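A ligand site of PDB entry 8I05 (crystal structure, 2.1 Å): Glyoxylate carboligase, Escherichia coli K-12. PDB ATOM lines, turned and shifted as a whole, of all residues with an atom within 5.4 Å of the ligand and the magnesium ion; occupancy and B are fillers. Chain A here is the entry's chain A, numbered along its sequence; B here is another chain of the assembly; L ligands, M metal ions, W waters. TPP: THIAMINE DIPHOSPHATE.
A nitrogen (N4') of the ligand sits at hydrogen-bond distance from the backbone carbonyl oxygen (O) of Gly 420 (2.9 Å). The backbone NH (N) of Phe 448 sits close to an oxygen (O2A) of the ligand. N of Ser 397 lies within hydrogen-bond range of O2B of the ligand, at 3.0 Å. The side-chain amide nitrogen (NE2) of Gln 116 of chain B sits close to a nitrogen (N4') of the ligand. O3B of the ligand sits at hydrogen-bond distance from N of Gly 478, at 3.3 Å. N of Asp 447 lies close to O2A of the ligand. The backbone NH of Leu 396 sits at hydrogen-bond distance from an oxygen (O3B) of the ligand (2.8 Å). N of Leu 479 lies within hydrogen-bond range of O3B of the ligand (2.9 Å). An oxygen (O1A) of the ligand sits at hydrogen-bond distance from the backbone NH (N) of Asp 449. A nitrogen (N3') of the ligand lies within hydrogen-bond range of the backbone NH (N) of Leu 422 (3.5 Å).
Water W4 lies within hydrogen-bond range of O2B of the ligand (2.8 Å), O of Val 472 (2.9 Å) and ND2 of Asn 474 (3.3 Å). Water W2 lies within hydrogen-bond range of O1A of the ligand, O of Ile 394, OG of Ser 397 and N of Gly 446. Water W1 lies within hydrogen-bond range of O2B of the ligand and ND2 of Asn 474. Water W3 lies within hydrogen-bond range of O of Val 26 of chain B, N of Thr 76 of chain B and N1' of the ligand.
Residues that only touch the ligand: Ile 394, Gly 395, Gly 446, Phe 452, Leu 477, Ile 480, Val 26 of chain B, Pro 27 of chain B, Val 52 of chain B, Thr 76 of chain B, Pro 79 of chain B and Asp 83 of chain B. Hydrophobic or aromatic side chains within 4 Å of the ligand: Ile 394, Leu 396, Leu 422, Phe 448, Phe 452, Leu 477, Leu 479, Ile 480, Val 26 of chain B, Val 52 of chain B and Pro 79 of chain B. The nearest printed residue that does not touch the ligand is Ala 80 of chain B (4.03 Å).
The magnesium ion is bound by the side-chain amide oxygen (OD1) of Asn 474 (2.0 Å), an oxygen (O2A) of the ligand (2.2 Å), the side-chain carboxylate (OD1) of Asp 447 (2.2 Å), the backbone carbonyl oxygen (O) of Tyr 476 (2.2 Å), an oxygen (O1B) of the ligand (2.3 Å) and water W4 (2.3 Å).
Three residues have an atom within 4 Å of the magnesium ion: Asp 447, Asn 474 and Tyr 476. The nearest printed residue that does not touch the magnesium ion is Gly 478 (4.1 Å).
OD2 of Asp 447 lies close to OD1 of Asn 473, 3.2 Å away. The side-chain amide nitrogen (NE2) of Gln 116 of chain B is in hydrogen-bond range of the backbone carbonyl oxygen (O) of Ala 419 (2.7 Å). The side-chain carboxylate of Asp 449 sits at hydrogen-bond distance from the side-chain hydroxyl of Ser 445 (2.6 Å). The backbone carbonyl oxygen (O) of Gly 420 sits at hydrogen-bond distance from the side-chain amide nitrogen (NE2) of Gln 116 of chain B (3.2 Å). The backbone NH (N) of Gly 446 sits at hydrogen-bond distance from the side-chain hydroxyl (OG) of Ser 397. OD2 of Asp 447 lies within hydrogen-bond range of N of Ala 475, 3.2 Å away.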
ATOM      1  N   ILE A 394      13.915  -2.582  16.875  1.00  0.00           N
ATOM      2  CA  ILE A 394      14.179  -2.177  18.258  1.00  0.00           C
ATOM      3  C   ILE A 394      15.666  -2.328  18.523  1.00  0.00           C
ATOM      4  O   ILE A 394      16.371  -3.056  17.809  1.00  0.00           O
ATOM      5  CB  ILE A 394      13.338  -3.030  19.247  1.00  0.00           C
ATOM      6  CG1 ILE A 394      13.333  -2.420  20.649  1.00  0.00           C
ATOM      7  CG2 ILE A 394      13.822  -4.479  19.272  1.00  0.00           C
ATOM      8  CD1 ILE A 394      12.361  -3.124  21.596  1.00  0.00           C
ATOM      9  N   GLY A 395      16.148  -1.683  19.584  1.00  0.00           N
ATOM     10  CA  GLY A 395      17.555  -1.625  19.922  1.00  0.00           C
ATOM     11  C   GLY A 395      18.078  -0.205  19.839  1.00  0.00           C
ATOM     12  O   GLY A 395      17.416   0.713  19.361  1.00  0.00           O
ATOM     13  N   LEU A 396      19.323  -0.047  20.298  1.00  0.00           N
ATOM     14  CA  LEU A 396      19.960   1.255  20.150  1.00  0.00           C
ATOM     15  C   LEU A 396      20.041   1.657  18.679  1.00  0.00           C
ATOM     16  O   LEU A 396      19.973   2.836  18.339  1.00  0.00           O
ATOM     17  CB  LEU A 396      21.347   1.238  20.793  1.00  0.00           C
ATOM     18  CG  LEU A 396      21.379   1.025  22.312  1.00  0.00           C
ATOM     19  CD1 LEU A 396      22.803   1.147  22.860  1.00  0.00           C
ATOM     20  CD2 LEU A 396      20.455   1.988  23.007  1.00  0.00           C
ATOM     21  N   SER A 397      20.143   0.664  17.798  1.00  0.00           N
ATOM     22  CA  SER A 397      20.098   0.901  16.367  1.00  0.00           C
ATOM     23  C   SER A 397      18.853   1.676  15.995  1.00  0.00           C
ATOM     24  O   SER A 397      18.918   2.706  15.305  1.00  0.00           O
ATOM     25  CB  SER A 397      20.106  -0.438  15.636  1.00  0.00           C
ATOM     26  OG  SER A 397      19.083  -1.271  16.215  1.00  0.00           O
ATOM     27  N   ALA A 419       5.269  -3.840  20.088  1.00  0.00           N
ATOM     28  CA  ALA A 419       5.737  -5.172  20.477  1.00  0.00           C
ATOM     29  C   ALA A 419       7.241  -5.364  20.287  1.00  0.00           C
ATOM     30  O   ALA A 419       7.874  -6.039  21.104  1.00  0.00           O
ATOM     31  CB  ALA A 419       5.001  -6.267  19.705  1.00  0.00           C
ATOM     32  N   GLY A 420       7.822  -4.813  19.217  1.00  0.00           N
ATOM     33  CA  GLY A 420       9.244  -4.862  19.011  1.00  0.00           C
ATOM     34  C   GLY A 420       9.915  -6.230  19.022  1.00  0.00           C
ATOM     35  O   GLY A 420      10.926  -6.415  19.701  1.00  0.00           O
ATOM     36  N   PRO A 421       9.388  -7.221  18.290  1.00  0.00           N
ATOM     37  CA  PRO A 421      10.042  -8.552  18.289  1.00  0.00           C
ATOM     38  C   PRO A 421      11.313  -8.553  17.465  1.00  0.00           C
ATOM     39  O   PRO A 421      11.302  -8.226  16.274  1.00  0.00           O
ATOM     40  CB  PRO A 421       8.992  -9.460  17.653  1.00  0.00           C
ATOM     41  CG  PRO A 421       8.179  -8.540  16.801  1.00  0.00           C
ATOM     42  CD  PRO A 421       8.153  -7.202  17.502  1.00  0.00           C
ATOM     43  N   LEU A 422      12.415  -9.000  18.072  1.00  0.00           N
ATOM     44  CA  LEU A 422      13.668  -9.148  17.345  1.00  0.00           C
ATOM     45  C   LEU A 422      13.472 -10.116  16.191  1.00  0.00           C
ATOM     46  O   LEU A 422      12.739 -11.091  16.324  1.00  0.00           O
ATOM     47  CB  LEU A 422      14.781  -9.636  18.285  1.00  0.00           C
ATOM     48  CG  LEU A 422      15.237  -8.600  19.327  1.00  0.00           C
ATOM     49  CD1 LEU A 422      16.149  -9.211  20.419  1.00  0.00           C
ATOM     50  CD2 LEU A 422      15.947  -7.427  18.621  1.00  0.00           C
ATOM     51  N   SER A 445      19.068  -2.530  11.229  1.00  0.00           N
ATOM     52  CA  SER A 445      19.127  -3.486  12.320  1.00  0.00           C
ATOM     53  C   SER A 445      20.418  -3.318  13.088  1.00  0.00           C
ATOM     54  O   SER A 445      21.448  -2.906  12.508  1.00  0.00           O
ATOM     55  CB  SER A 445      19.097  -4.963  11.846  1.00  0.00           C
ATOM     56  OG  SER A 445      17.896  -5.325  11.200  1.00  0.00           O
ATOM     57  N   GLY A 446      20.388  -3.683  14.387  1.00  0.00           N
ATOM     58  CA  GLY A 446      21.587  -4.096  15.090  1.00  0.00           C
ATOM     59  C   GLY A 446      21.945  -5.555  14.767  1.00  0.00           C
ATOM     60  O   GLY A 446      21.211  -6.256  14.080  1.00  0.00           O
ATOM     61  N   ASP A 447      23.107  -5.996  15.270  1.00  0.00           N
ATOM     62  CA  ASP A 447      23.566  -7.344  14.930  1.00  0.00           C
ATOM     63  C   ASP A 447      22.656  -8.433  15.516  1.00  0.00           C
ATOM     64  O   ASP A 447      22.380  -9.429  14.843  1.00  0.00           O
ATOM     65  CB  ASP A 447      25.030  -7.553  15.345  1.00  0.00           C
ATOM     66  CG  ASP A 447      25.370  -6.964  16.702  1.00  0.00           C
ATOM     67  OD1 ASP A 447      24.933  -5.820  17.010  1.00  0.00           O
ATOM     68  OD2 ASP A 447      26.086  -7.644  17.463  1.00  0.00           O
ATOM     69  N   PHE A 448      22.116  -8.233  16.716  1.00  0.00           N
ATOM     70  CA  PHE A 448      21.288  -9.265  17.346  1.00  0.00           C
ATOM     71  C   PHE A 448      19.963  -9.401  16.604  1.00  0.00           C
ATOM     72  O   PHE A 448      19.593 -10.509  16.193  1.00  0.00           O
ATOM     73  CB  PHE A 448      21.059  -8.918  18.825  1.00  0.00           C
ATOM     74  CG  PHE A 448      20.677 -10.103  19.705  1.00  0.00           C
ATOM     75  CD1 PHE A 448      21.433 -11.287  19.705  1.00  0.00           C
ATOM     76  CD2 PHE A 448      19.624  -9.994  20.597  1.00  0.00           C
ATOM     77  CE1 PHE A 448      21.109 -12.344  20.539  1.00  0.00           C
ATOM     78  CE2 PHE A 448      19.290 -11.047  21.429  1.00  0.00           C
ATOM     79  CZ  PHE A 448      20.044 -12.244  21.411  1.00  0.00           C
ATOM     80  N   ASP A 449      19.271  -8.278  16.365  1.00  0.00           N
ATOM     81  CA  ASP A 449      18.074  -8.291  15.528  1.00  0.00           C
ATOM     82  C   ASP A 449      18.345  -8.994  14.205  1.00  0.00           C
ATOM     83  O   ASP A 449      17.562  -9.843  13.757  1.00  0.00           O
ATOM     84  CB  ASP A 449      17.583  -6.856  15.286  1.00  0.00           C
ATOM     85  CG  ASP A 449      16.442  -6.745  14.249  1.00  0.00           C
ATOM     86  OD1 ASP A 449      15.463  -7.528  14.286  1.00  0.00           O
ATOM     87  OD2 ASP A 449      16.505  -5.836  13.396  1.00  0.00           O
ATOM     88  N   PHE A 450      19.475  -8.648  13.581  1.00  0.00           N
ATOM     89  CA  PHE A 450      19.772  -9.199  12.270  1.00  0.00           C
ATOM     90  C   PHE A 450      19.943 -10.724  12.304  1.00  0.00           C
ATOM     91  O   PHE A 450      19.567 -11.412  11.363  1.00  0.00           O
ATOM     92  CB  PHE A 450      21.035  -8.519  11.722  1.00  0.00           C
ATOM     93  CG  PHE A 450      21.308  -8.774  10.267  1.00  0.00           C
ATOM     94  CD1 PHE A 450      20.563  -8.163   9.290  1.00  0.00           C
ATOM     95  CD2 PHE A 450      22.361  -9.593   9.893  1.00  0.00           C
ATOM     96  CE1 PHE A 450      20.852  -8.388   7.959  1.00  0.00           C
ATOM     97  CE2 PHE A 450      22.644  -9.811   8.552  1.00  0.00           C
ATOM     98  CZ  PHE A 450      21.897  -9.224   7.597  1.00  0.00           C
ATOM     99  N   PHE A 452      18.427 -13.026  14.412  1.00  0.00           N
ATOM    100  CA  PHE A 452      17.263 -13.851  14.785  1.00  0.00           C
ATOM    101  C   PHE A 452      16.690 -14.608  13.593  1.00  0.00           C
ATOM    102  O   PHE A 452      16.478 -15.826  13.657  1.00  0.00           O
ATOM    103  CB  PHE A 452      16.163 -12.979  15.400  1.00  0.00           C
ATOM    104  CG  PHE A 452      16.123 -12.962  16.913  1.00  0.00           C
ATOM    105  CD1 PHE A 452      17.230 -12.586  17.649  1.00  0.00           C
ATOM    106  CD2 PHE A 452      14.949 -13.265  17.589  1.00  0.00           C
ATOM    107  CE1 PHE A 452      17.184 -12.546  19.043  1.00  0.00           C
ATOM    108  CE2 PHE A 452      14.897 -13.217  18.973  1.00  0.00           C
ATOM    109  CZ  PHE A 452      16.019 -12.861  19.694  1.00  0.00           C
ATOM    110  N   VAL A 472      24.265  -2.280  11.796  1.00  0.00           N
ATOM    111  CA  VAL A 472      25.205  -1.572  12.647  1.00  0.00           C
ATOM    112  C   VAL A 472      25.614  -2.540  13.758  1.00  0.00           C
ATOM    113  O   VAL A 472      24.790  -2.945  14.585  1.00  0.00           O
ATOM    114  CB  VAL A 472      24.640  -0.235  13.167  1.00  0.00           C
ATOM    115  CG1 VAL A 472      24.407   0.719  12.005  1.00  0.00           C
ATOM    116  CG2 VAL A 472      23.320  -0.393  13.899  1.00  0.00           C
ATOM    117  N   ASN A 473      26.884  -2.925  13.757  1.00  0.00           N
ATOM    118  CA  ASN A 473      27.362  -4.098  14.503  1.00  0.00           C
ATOM    119  C   ASN A 473      28.250  -3.630  15.651  1.00  0.00           C
ATOM    120  O   ASN A 473      29.372  -3.157  15.431  1.00  0.00           O
ATOM    121  CB  ASN A 473      28.115  -5.038  13.553  1.00  0.00           C
ATOM    122  CG  ASN A 473      28.661  -6.302  14.255  1.00  0.00           C
ATOM    123  OD1 ASN A 473      28.356  -6.562  15.418  1.00  0.00           O
ATOM    124  ND2 ASN A 473      29.477  -7.078  13.544  1.00  0.00           N
ATOM    125  N   ASN A 474      27.758  -3.762  16.882  1.00  0.00           N
ATOM    126  CA  ASN A 474      28.577  -3.510  18.065  1.00  0.00           C
ATOM    127  C   ASN A 474      28.954  -4.793  18.829  1.00  0.00           C
ATOM    128  O   ASN A 474      29.530  -4.695  19.914  1.00  0.00           O
ATOM    129  CB  ASN A 474      27.870  -2.519  18.985  1.00  0.00           C
ATOM    130  CG  ASN A 474      26.419  -2.911  19.306  1.00  0.00           C
ATOM    131  OD1 ASN A 474      26.025  -4.075  19.127  1.00  0.00           O
ATOM    132  ND2 ASN A 474      25.626  -1.945  19.781  1.00  0.00           N
ATOM    133  N   ALA A 475      28.637  -5.977  18.295  1.00  0.00           N
ATOM    134  CA  ALA A 475      28.828  -7.261  18.995  1.00  0.00           C
ATOM    135  C   ALA A 475      28.216  -7.246  20.407  1.00  0.00           C
ATOM    136  O   ALA A 475      28.749  -7.859  21.335  1.00  0.00           O
ATOM    137  CB  ALA A 475      30.303  -7.657  19.046  1.00  0.00           C
ATOM    138  N   TYR A 476      27.077  -6.584  20.561  1.00  0.00           N
ATOM    139  CA  TYR A 476      26.423  -6.417  21.858  1.00  0.00           C
ATOM    140  C   TYR A 476      24.921  -6.469  21.665  1.00  0.00           C
ATOM    141  O   TYR A 476      24.418  -6.102  20.606  1.00  0.00           O
ATOM    142  CB  TYR A 476      26.756  -5.051  22.484  1.00  0.00           C
ATOM    143  CG  TYR A 476      27.718  -4.964  23.648  1.00  0.00           C
ATOM    144  CD1 TYR A 476      27.319  -5.309  24.925  1.00  0.00           C
ATOM    145  CD2 TYR A 476      28.998  -4.459  23.474  1.00  0.00           C
ATOM    146  CE1 TYR A 476      28.193  -5.177  25.999  1.00  0.00           C
ATOM    147  CE2 TYR A 476      29.880  -4.336  24.536  1.00  0.00           C
ATOM    148  CZ  TYR A 476      29.467  -4.693  25.802  1.00  0.00           C
ATOM    149  OH  TYR A 476      30.323  -4.579  26.874  1.00  0.00           O
ATOM    150  N   LEU A 477      24.187  -6.897  22.708  1.00  0.00           N
ATOM    151  CA  LEU A 477      22.788  -6.483  22.853  1.00  0.00           C
ATOM    152  C   LEU A 477      22.827  -5.094  23.473  1.00  0.00           C
ATOM    153  O   LEU A 477      22.780  -4.929  24.694  1.00  0.00           O
ATOM    154  CB  LEU A 477      21.985  -7.442  23.734  1.00  0.00           C
ATOM    155  CG  LEU A 477      22.146  -8.963  23.767  1.00  0.00           C
ATOM    156  CD1 LEU A 477      20.886  -9.635  24.320  1.00  0.00           C
ATOM    157  CD2 LEU A 477      22.542  -9.547  22.439  1.00  0.00           C
ATOM    158  N   GLY A 478      22.959  -4.063  22.621  1.00  0.00           N
ATOM    159  CA  GLY A 478      23.350  -2.761  23.120  1.00  0.00           C
ATOM    160  C   GLY A 478      22.309  -2.104  24.011  1.00  0.00           C
ATOM    161  O   GLY A 478      22.638  -1.548  25.060  1.00  0.00           O
ATOM    162  N   LEU A 479      21.036  -2.193  23.634  1.00  0.00           N
ATOM    163  CA  LEU A 479      19.992  -1.615  24.475  1.00  0.00           C
ATOM    164  C   LEU A 479      19.972  -2.280  25.853  1.00  0.00           C
ATOM    165  O   LEU A 479      19.711  -1.592  26.848  1.00  0.00           O
ATOM    166  CB  LEU A 479      18.627  -1.744  23.805  1.00  0.00           C
ATOM    167  CG  LEU A 479      17.419  -1.104  24.527  1.00  0.00           C
ATOM    168  CD1 LEU A 479      17.731   0.333  24.961  1.00  0.00           C
ATOM    169  CD2 LEU A 479      16.154  -1.161  23.659  1.00  0.00           C
ATOM    170  N   ILE A 480      20.292  -3.573  25.944  1.00  0.00           N
ATOM    171  CA  ILE A 480      20.201  -4.255  27.244  1.00  0.00           C
ATOM    172  C   ILE A 480      21.422  -3.963  28.083  1.00  0.00           C
ATOM    173  O   ILE A 480      21.326  -3.837  29.316  1.00  0.00           O
ATOM    174  CB  ILE A 480      19.980  -5.770  27.081  1.00  0.00           C
ATOM    175  CG1 ILE A 480      18.835  -6.040  26.081  1.00  0.00           C
ATOM    176  CG2 ILE A 480      19.673  -6.424  28.449  1.00  0.00           C
ATOM    177  CD1 ILE A 480      17.573  -5.195  26.317  1.00  0.00           C
ATOM    178  N   LEU A 495      28.139 -10.508  22.318  1.00  0.00           N
ATOM    179  CA  LEU A 495      28.103 -11.485  21.237  1.00  0.00           C
ATOM    180  C   LEU A 495      29.481 -11.740  20.627  1.00  0.00           C
ATOM    181  O   LEU A 495      29.588 -12.570  19.710  1.00  0.00           O
ATOM    182  CB  LEU A 495      27.128 -11.028  20.155  1.00  0.00           C
ATOM    183  CG  LEU A 495      25.673 -10.884  20.627  1.00  0.00           C
ATOM    184  CD1 LEU A 495      24.877 -10.121  19.601  1.00  0.00           C
ATOM    185  CD2 LEU A 495      25.030 -12.271  20.882  1.00  0.00           C
ATOM    186  N   VAL B  26      17.709 -14.988  26.750  1.00  0.00           N
ATOM    187  CA  VAL B  26      17.983 -13.720  26.093  1.00  0.00           C
ATOM    188  C   VAL B  26      17.523 -12.635  27.072  1.00  0.00           C
ATOM    189  O   VAL B  26      16.322 -12.551  27.346  1.00  0.00           O
ATOM    190  CB  VAL B  26      17.254 -13.586  24.754  1.00  0.00           C
ATOM    191  CG1 VAL B  26      17.473 -12.172  24.126  1.00  0.00           C
ATOM    192  CG2 VAL B  26      17.661 -14.693  23.782  1.00  0.00           C
ATOM    193  N   PRO B  27      18.421 -11.834  27.641  1.00  0.00           N
ATOM    194  CA  PRO B  27      18.003 -10.813  28.603  1.00  0.00           C
ATOM    195  C   PRO B  27      17.266  -9.667  27.919  1.00  0.00           C
ATOM    196  O   PRO B  27      17.319  -9.493  26.688  1.00  0.00           O
ATOM    197  CB  PRO B  27      19.326 -10.323  29.212  1.00  0.00           C
ATOM    198  CG  PRO B  27      20.311 -10.579  28.158  1.00  0.00           C
ATOM    199  CD  PRO B  27      19.892 -11.831  27.465  1.00  0.00           C
ATOM    200  N   GLY B  28      16.549  -8.903  28.739  1.00  0.00           N
ATOM    201  CA  GLY B  28      15.909  -7.664  28.317  1.00  0.00           C
ATOM    202  C   GLY B  28      15.606  -6.852  29.554  1.00  0.00           C
ATOM    203  O   GLY B  28      15.740  -7.334  30.678  1.00  0.00           O
ATOM    204  N   VAL B  52      15.007 -16.202  20.802  1.00  0.00           N
ATOM    205  CA  VAL B  52      14.366 -16.717  22.008  1.00  0.00           C
ATOM    206  C   VAL B  52      13.834 -18.125  21.747  1.00  0.00           C
ATOM    207  O   VAL B  52      13.865 -18.972  22.649  1.00  0.00           O
ATOM    208  CB  VAL B  52      13.269 -15.748  22.498  1.00  0.00           C
ATOM    209  CG1 VAL B  52      12.386 -16.430  23.565  1.00  0.00           C
ATOM    210  CG2 VAL B  52      13.915 -14.507  23.088  1.00  0.00           C
ATOM    211  N   THR B  76      12.589 -11.793  28.273  1.00  0.00           N
ATOM    212  CA  THR B  76      12.013 -10.531  28.742  1.00  0.00           C
ATOM    213  C   THR B  76      10.495 -10.556  28.510  1.00  0.00           C
ATOM    214  O   THR B  76       9.907 -11.599  28.207  1.00  0.00           O
ATOM    215  CB  THR B  76      12.726  -9.346  28.054  1.00  0.00           C
ATOM    216  OG1 THR B  76      12.459  -8.145  28.771  1.00  0.00           O
ATOM    217  CG2 THR B  76      12.273  -9.155  26.615  1.00  0.00           C
ATOM    218  N   PRO B  79       7.337  -9.935  23.322  1.00  0.00           N
ATOM    219  CA  PRO B  79       7.569 -10.957  22.297  1.00  0.00           C
ATOM    220  C   PRO B  79       8.457 -12.114  22.736  1.00  0.00           C
ATOM    221  O   PRO B  79       8.474 -13.138  22.055  1.00  0.00           O
ATOM    222  CB  PRO B  79       8.201 -10.176  21.134  1.00  0.00           C
ATOM    223  CG  PRO B  79       8.879  -9.044  21.810  1.00  0.00           C
ATOM    224  CD  PRO B  79       8.001  -8.663  22.984  1.00  0.00           C
ATOM    225  N   ALA B  80       9.248 -11.975  23.798  1.00  0.00           N
ATOM    226  CA  ALA B  80      10.002 -13.130  24.263  1.00  0.00           C
ATOM    227  C   ALA B  80       9.066 -14.262  24.693  1.00  0.00           C
ATOM    228  O   ALA B  80       9.238 -15.403  24.274  1.00  0.00           O
ATOM    229  CB  ALA B  80      10.939 -12.729  25.418  1.00  0.00           C
ATOM    230  N   ASP B  83       7.476 -15.928  21.740  1.00  0.00           N
ATOM    231  CA  ASP B  83       8.460 -16.761  21.058  1.00  0.00           C
ATOM    232  C   ASP B  83       8.704 -18.096  21.775  1.00  0.00           C
ATOM    233  O   ASP B  83       9.428 -18.935  21.223  1.00  0.00           O
ATOM    234  CB  ASP B  83       9.795 -16.036  20.950  1.00  0.00           C
ATOM    235  CG  ASP B  83       9.860 -15.052  19.763  1.00  0.00           C
ATOM    236  OD1 ASP B  83       8.935 -14.996  18.888  1.00  0.00           O
ATOM    237  OD2 ASP B  83      10.885 -14.340  19.741  1.00  0.00           O
ATOM    238  N   GLN B 116       5.658  -3.355  25.235  1.00  0.00           N
ATOM    239  CA  GLN B 116       6.063  -4.767  25.239  1.00  0.00           C
ATOM    240  C   GLN B 116       5.468  -5.562  26.408  1.00  0.00           C
ATOM    241  O   GLN B 116       6.161  -6.338  27.057  1.00  0.00           O
ATOM    242  CB  GLN B 116       7.590  -4.911  25.243  1.00  0.00           C
ATOM    243  CG  GLN B 116       8.292  -4.516  23.965  1.00  0.00           C
ATOM    244  CD  GLN B 116       9.720  -5.063  23.847  1.00  0.00           C
ATOM    245  OE1 GLN B 116      10.527  -4.960  24.781  1.00  0.00           O
ATOM    246  NE2 GLN B 116      10.027  -5.645  22.687  1.00  0.00           N
HETATM  247  N1' TPP L   1      13.672 -10.870  22.905  1.00  0.00           N
HETATM  248  C2' TPP L   1      12.859 -10.528  21.892  1.00  0.00           C
HETATM  249  CM2 TPP L   1      12.236 -11.643  21.115  1.00  0.00           C
HETATM  250  N3' TPP L   1      12.537  -9.284  21.534  1.00  0.00           N
HETATM  251  C4' TPP L   1      13.088  -8.275  22.224  1.00  0.00           C
HETATM  252  N4' TPP L   1      12.770  -7.035  21.831  1.00  0.00           N
HETATM  253  C5' TPP L   1      13.999  -8.514  23.296  1.00  0.00           C
HETATM  254  C6' TPP L   1      14.229  -9.854  23.578  1.00  0.00           C
HETATM  255  C7' TPP L   1      14.647  -7.427  24.127  1.00  0.00           C
HETATM  256  N3  TPP L   1      15.604  -6.574  23.386  1.00  0.00           N
HETATM  257  C2  TPP L   1      15.304  -5.370  22.922  1.00  0.00           C
HETATM  258  S1  TPP L   1      16.604  -4.625  22.140  1.00  0.00           S
HETATM  259  C5  TPP L   1      17.622  -5.978  22.495  1.00  0.00           C
HETATM  260  C4  TPP L   1      16.930  -6.954  23.162  1.00  0.00           C
HETATM  261  CM4 TPP L   1      17.444  -8.276  23.629  1.00  0.00           C
HETATM  262  C6  TPP L   1      19.029  -5.981  21.993  1.00  0.00           C
HETATM  263  C7  TPP L   1      19.088  -5.691  20.518  1.00  0.00           C
HETATM  264  O7  TPP L   1      20.463  -5.666  20.089  1.00  0.00           O
HETATM  265  PA  TPP L   1      20.909  -5.330  18.615  1.00  0.00           P
HETATM  266  O1A TPP L   1      19.778  -5.729  17.686  1.00  0.00           O
HETATM  267  O2A TPP L   1      22.304  -5.788  18.448  1.00  0.00           O
HETATM  268  O3A TPP L   1      20.919  -3.767  18.788  1.00  0.00           O
HETATM  269  PB  TPP L   1      21.774  -2.695  19.576  1.00  0.00           P
HETATM  270  O1B TPP L   1      23.031  -3.345  20.057  1.00  0.00           O
HETATM  271  O2B TPP L   1      21.987  -1.547  18.563  1.00  0.00           O
HETATM  272  O3B TPP L   1      20.883  -2.270  20.743  1.00  0.00           O
HETATM  273 MG    MG M   1      24.216  -4.862  18.815  1.00  0.00          MG
HETATM  274  O   HOH W   1      23.911   0.474  17.953  1.00  0.00           O
HETATM  275  O   HOH W   2      18.424  -3.894  16.336  1.00  0.00           O
HETATM  276  O   HOH W   3      14.105 -12.122  25.764  1.00  0.00           O
HETATM  277  O   HOH W   4      23.884  -3.114  17.292  1.00  0.00           O
